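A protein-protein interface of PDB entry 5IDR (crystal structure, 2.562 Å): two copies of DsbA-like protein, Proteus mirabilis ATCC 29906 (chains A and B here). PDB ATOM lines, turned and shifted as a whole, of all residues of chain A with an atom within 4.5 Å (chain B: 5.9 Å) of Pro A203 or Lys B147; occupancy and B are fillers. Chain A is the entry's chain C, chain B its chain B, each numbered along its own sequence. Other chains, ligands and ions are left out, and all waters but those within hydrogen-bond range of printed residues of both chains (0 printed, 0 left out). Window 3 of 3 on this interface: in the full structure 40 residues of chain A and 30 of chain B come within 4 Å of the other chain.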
ATOM      1  N   GLY A 188       2.798  10.819  18.245  1.00  0.00           N
ATOM      2  CA  GLY A 188       3.347  11.313  16.994  1.00  0.00           C
ATOM      3  C   GLY A 188       2.453  12.327  16.307  1.00  0.00           C
ATOM      4  O   GLY A 188       2.538  12.503  15.091  1.00  0.00           O
ATOM      5  N   ILE A 189       1.599  12.984  17.084  1.00  0.00           N
ATOM      6  CA  ILE A 189       0.694  14.006  16.564  1.00  0.00           C
ATOM      7  C   ILE A 189       1.357  15.387  16.593  1.00  0.00           C
ATOM      8  O   ILE A 189       1.481  16.000  17.657  1.00  0.00           O
ATOM      9  CB  ILE A 189      -0.627  14.047  17.372  1.00  0.00           C
ATOM     10  CG1 ILE A 189      -1.431  12.774  17.119  1.00  0.00           C
ATOM     11  CG2 ILE A 189      -1.475  15.249  16.966  1.00  0.00           C
ATOM     12  CD1 ILE A 189      -2.693  12.639  18.003  1.00  0.00           C
ATOM     13  N   GLN A 190       1.749  15.875  15.414  1.00  0.00           N
ATOM     14  CA  GLN A 190       2.524  17.111  15.283  1.00  0.00           C
ATOM     15  C   GLN A 190       1.694  18.270  14.754  1.00  0.00           C
ATOM     16  O   GLN A 190       2.192  19.396  14.630  1.00  0.00           O
ATOM     17  CB  GLN A 190       3.722  16.915  14.338  1.00  0.00           C
ATOM     18  CG  GLN A 190       4.605  15.727  14.641  1.00  0.00           C
ATOM     19  CD  GLN A 190       5.042  15.673  16.077  1.00  0.00           C
ATOM     20  OE1 GLN A 190       4.685  14.752  16.803  1.00  0.00           O
ATOM     21  NE2 GLN A 190       5.841  16.641  16.494  1.00  0.00           N
ATOM     22  N   GLY A 191       0.442  17.997  14.410  1.00  0.00           N
ATOM     23  CA  GLY A 191      -0.410  19.008  13.812  1.00  0.00           C
ATOM     24  C   GLY A 191      -1.870  18.747  14.081  1.00  0.00           C
ATOM     25  O   GLY A 191      -2.246  17.704  14.613  1.00  0.00           O
ATOM     26  N   THR A 192      -2.692  19.713  13.698  1.00  0.00           N
ATOM     27  CA  THR A 192      -4.122  19.654  13.942  1.00  0.00           C
ATOM     28  C   THR A 192      -4.910  19.906  12.665  1.00  0.00           C
ATOM     29  O   THR A 192      -4.460  20.658  11.796  1.00  0.00           O
ATOM     30  CB  THR A 192      -4.536  20.692  14.999  1.00  0.00           C
ATOM     31  OG1 THR A 192      -4.140  22.003  14.565  1.00  0.00           O
ATOM     32  CG2 THR A 192      -3.886  20.392  16.352  1.00  0.00           C
ATOM     33  N   PRO A 193      -6.099  19.288  12.544  1.00  0.00           N
ATOM     34  CA  PRO A 193      -6.668  18.325  13.492  1.00  0.00           C
ATOM     35  C   PRO A 193      -6.099  16.934  13.328  1.00  0.00           C
ATOM     36  O   PRO A 193      -5.594  16.590  12.260  1.00  0.00           O
ATOM     37  CB  PRO A 193      -8.158  18.324  13.142  1.00  0.00           C
ATOM     38  CG  PRO A 193      -8.208  18.691  11.722  1.00  0.00           C
ATOM     39  CD  PRO A 193      -7.081  19.665  11.508  1.00  0.00           C
ATOM     40  N   ILE A 201      -5.409   6.637  13.905  1.00  0.00           N
ATOM     41  CA  ILE A 201      -5.363   8.090  14.043  1.00  0.00           C
ATOM     42  C   ILE A 201      -5.656   8.751  12.702  1.00  0.00           C
ATOM     43  O   ILE A 201      -4.895   8.605  11.759  1.00  0.00           O
ATOM     44  CB  ILE A 201      -4.000   8.572  14.552  1.00  0.00           C
ATOM     45  CG1 ILE A 201      -3.715   7.976  15.927  1.00  0.00           C
ATOM     46  CG2 ILE A 201      -3.970  10.090  14.639  1.00  0.00           C
ATOM     47  CD1 ILE A 201      -2.362   8.391  16.507  1.00  0.00           C
ATOM     48  N   LEU A 202      -6.758   9.485  12.629  1.00  0.00           N
ATOM     49  CA  LEU A 202      -7.183  10.101  11.384  1.00  0.00           C
ATOM     50  C   LEU A 202      -6.478  11.444  11.218  1.00  0.00           C
ATOM     51  O   LEU A 202      -6.714  12.377  11.973  1.00  0.00           O
ATOM     52  CB  LEU A 202      -8.696  10.256  11.373  1.00  0.00           C
ATOM     53  CG  LEU A 202      -9.348  10.535  10.027  1.00  0.00           C
ATOM     54  CD1 LEU A 202      -9.079   9.392   9.077  1.00  0.00           C
ATOM     55  CD2 LEU A 202     -10.841  10.735  10.212  1.00  0.00           C
ATOM     56  N   PRO A 203      -5.588  11.540  10.235  1.00  0.00           N
ATOM     57  CA  PRO A 203      -4.631  12.643  10.267  1.00  0.00           C
ATOM     58  C   PRO A 203      -5.048  13.932   9.570  1.00  0.00           C
ATOM     59  O   PRO A 203      -4.190  14.599   9.014  1.00  0.00           O
ATOM     60  CB  PRO A 203      -3.420  12.032   9.564  1.00  0.00           C
ATOM     61  CG  PRO A 203      -4.018  11.140   8.555  1.00  0.00           C
ATOM     62  CD  PRO A 203      -5.219  10.536   9.220  1.00  0.00           C
ATOM     63  N   GLY A 204      -6.314  14.308   9.600  1.00  0.00           N
ATOM     64  CA  GLY A 204      -6.658  15.684   9.256  1.00  0.00           C
ATOM     65  C   GLY A 204      -8.150  15.986   9.243  1.00  0.00           C
ATOM     66  O   GLY A 204      -8.945  15.350   9.943  1.00  0.00           O
ATOM     67  N   LYS B  88       5.234  24.305  11.939  1.00  0.00           N
ATOM     68  CA  LYS B  88       4.238  24.023  10.915  1.00  0.00           C
ATOM     69  C   LYS B  88       3.218  25.152  10.849  1.00  0.00           C
ATOM     70  O   LYS B  88       2.636  25.435   9.801  1.00  0.00           O
ATOM     71  CB  LYS B  88       3.542  22.692  11.203  1.00  0.00           C
ATOM     72  CG  LYS B  88       4.427  21.451  11.019  1.00  0.00           C
ATOM     73  CD  LYS B  88       3.613  20.186  11.252  1.00  0.00           C
ATOM     74  CE  LYS B  88       4.427  18.948  11.147  1.00  0.00           C
ATOM     75  NZ  LYS B  88       4.491  18.513   9.733  1.00  0.00           N
ATOM     76  N   ARG B  89       3.022  25.806  11.981  1.00  0.00           N
ATOM     77  CA  ARG B  89       2.042  26.869  12.086  1.00  0.00           C
ATOM     78  C   ARG B  89       2.632  28.258  11.889  1.00  0.00           C
ATOM     79  O   ARG B  89       1.932  29.177  11.477  1.00  0.00           O
ATOM     80  CB  ARG B  89       1.351  26.774  13.441  1.00  0.00           C
ATOM     81  CG  ARG B  89       0.426  25.565  13.519  1.00  0.00           C
ATOM     82  CD  ARG B  89      -0.841  25.833  12.731  1.00  0.00           C
ATOM     83  NE  ARG B  89      -1.516  24.607  12.337  1.00  0.00           N
ATOM     84  CZ  ARG B  89      -2.641  24.586  11.637  1.00  0.00           C
ATOM     85  NH1 ARG B  89      -3.197  25.731  11.257  1.00  0.00           N
ATOM     86  NH2 ARG B  89      -3.200  23.425  11.311  1.00  0.00           N
ATOM     87  N   MET B 144       5.126  20.666   5.710  1.00  0.00           N
ATOM     88  CA  MET B 144       4.657  21.426   6.857  1.00  0.00           C
ATOM     89  C   MET B 144       3.218  21.067   7.194  1.00  0.00           C
ATOM     90  O   MET B 144       2.831  21.113   8.357  1.00  0.00           O
ATOM     91  CB  MET B 144       4.784  22.926   6.604  1.00  0.00           C
ATOM     92  CG  MET B 144       6.196  23.430   6.692  1.00  0.00           C
ATOM     93  SD  MET B 144       6.935  23.132   8.312  1.00  0.00           S
ATOM     94  CE  MET B 144       8.311  24.262   8.231  1.00  0.00           C
ATOM     95  N   GLN B 145       2.441  20.687   6.183  1.00  0.00           N
ATOM     96  CA  GLN B 145       1.047  20.270   6.388  1.00  0.00           C
ATOM     97  C   GLN B 145       0.871  18.876   6.999  1.00  0.00           C
ATOM     98  O   GLN B 145      -0.206  18.565   7.497  1.00  0.00           O
ATOM     99  CB  GLN B 145       0.277  20.295   5.070  1.00  0.00           C
ATOM    100  CG  GLN B 145      -0.057  21.676   4.558  1.00  0.00           C
ATOM    101  CD  GLN B 145      -0.334  21.668   3.073  1.00  0.00           C
ATOM    102  OE1 GLN B 145      -0.753  20.647   2.510  1.00  0.00           O
ATOM    103  NE2 GLN B 145      -0.083  22.803   2.420  1.00  0.00           N
ATOM    104  N   LYS B 146       1.883  18.015   6.944  1.00  0.00           N
ATOM    105  CA  LYS B 146       1.727  16.701   7.562  1.00  0.00           C
ATOM    106  C   LYS B 146       1.429  16.876   9.053  1.00  0.00           C
ATOM    107  O   LYS B 146       2.139  17.595   9.750  1.00  0.00           O
ATOM    108  CB  LYS B 146       2.972  15.842   7.343  1.00  0.00           C
ATOM    109  CG  LYS B 146       3.202  15.500   5.887  1.00  0.00           C
ATOM    110  CD  LYS B 146       2.453  14.269   5.479  1.00  0.00           C
ATOM    111  CE  LYS B 146       2.628  13.971   4.004  1.00  0.00           C
ATOM    112  NZ  LYS B 146       1.881  12.733   3.614  1.00  0.00           N
ATOM    113  N   LYS B 147       0.358  16.242   9.525  1.00  0.00           N
ATOM    114  CA  LYS B 147      -0.053  16.361  10.921  1.00  0.00           C
ATOM    115  C   LYS B 147       0.634  15.313  11.801  1.00  0.00           C
ATOM    116  O   LYS B 147       0.596  15.374  13.031  1.00  0.00           O
ATOM    117  CB  LYS B 147      -1.576  16.220  11.045  1.00  0.00           C
ATOM    118  CG  LYS B 147      -2.399  16.939   9.974  1.00  0.00           C
ATOM    119  CD  LYS B 147      -2.366  18.452  10.117  1.00  0.00           C
ATOM    120  CE  LYS B 147      -3.164  19.104   8.989  1.00  0.00           C
ATOM    121  NZ  LYS B 147      -3.264  20.596   9.128  1.00  0.00           N
ATOM    122  N   THR B 148       1.253  14.349  11.149  1.00  0.00           N
ATOM    123  CA  THR B 148       1.847  13.195  11.807  1.00  0.00           C
ATOM    124  C   THR B 148       3.377  13.247  11.719  1.00  0.00           C
ATOM    125  O   THR B 148       3.935  13.895  10.817  1.00  0.00           O
ATOM    126  CB  THR B 148       1.266  11.922  11.166  1.00  0.00           C
ATOM    127  OG1 THR B 148      -0.018  11.685  11.755  1.00  0.00           O
ATOM    128  CG2 THR B 148       2.158  10.700  11.346  1.00  0.00           C
ATOM    129  N   MET B 149       4.055  12.614  12.678  1.00  0.00           N
ATOM    130  CA  MET B 149       5.508  12.494  12.613  1.00  0.00           C
ATOM    131  C   MET B 149       5.863  11.934  11.263  1.00  0.00           C
ATOM    132  O   MET B 149       5.323  10.907  10.847  1.00  0.00           O
ATOM    133  CB  MET B 149       6.071  11.585  13.704  1.00  0.00           C
ATOM    134  CG  MET B 149       6.559  12.313  14.953  1.00  0.00           C
ATOM    135  SD  MET B 149       7.951  13.430  14.683  1.00  0.00           S
ATOM    136  CE  MET B 149       9.127  12.322  13.951  1.00  0.00           C
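NH2 of Arg B89 sits at hydrogen-bond distance from O of Thr A192 (3.1 Å). N of Gln A190 is in hydrogen-bond range of O of Lys B147 (2.7 Å). The backbone carbonyl oxygen (O) of Lys B147 is in hydrogen-bond range of the backbone NH (N) of Gly A191, 3.0 Å away. NZ of Lys B147 sits at hydrogen-bond distance from O of Thr A192, 2.9 Å away. N of Met B149 is in hydrogen-bond range of O of Gly A188, at 2.9 Å.
The backbone carbonyl oxygen of Met B144 lies close to the side-chain amino group of Lys B88, at 3.4 Å. NZ of Lys B88 lies within hydrogen-bond range of O of Lys B146, 2.5 Å away.
Among the printed residues, merely in contact across the chains: Pro A203 with Lys B147 (3.1 Å), Gly A188 with Thr B148 (3.4 Å), Gln A190 with Met B149 (3.6 Å), Ile A189 with Lys B147 (3.6 Å), Gln A190 with Lys B88 (3.7 Å) and Pro A193 with Lys B147 (3.9 Å).
Of chain A, only Ile A189 (3.6 Å), Gln A190 (2.7 Å), Gly A191 (3.0 Å), Thr A192 (2.9 Å), Pro A193 (3.9 Å) and Pro A203 (3.1 Å) come within 4 Å of Lys B147. Of the printed residues of chain B, Gly A191 touches Lys B147. Printed residues of chain B within 4 Å of Pro A193: Lys B147 (3.9 Å). Lys B146 touches none of the printed residues of chain A. Met B144 touches none of the printed residues of chain A. The nearest residue of chain B that does not touch Pro A203 is Thr B148 (4.1 Å). The nearest printed residue of chain B that does not touch Gly A191 is Lys B88 (4.9 Å).
Of the 10 printed residues of chain A, 7 touch a printed residue of chain B. Printed residues of chain A that touch a printed residue of chain B: Gly A188, Ile A189, Gln A190, Gly A191, Thr A192, Pro A193 and Pro A203. Among the printed residues, no Asp or Glu carboxylate lies within 4 Å of a Lys or Arg side-chain nitrogen of the other chain.
No position is printed for both chains.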
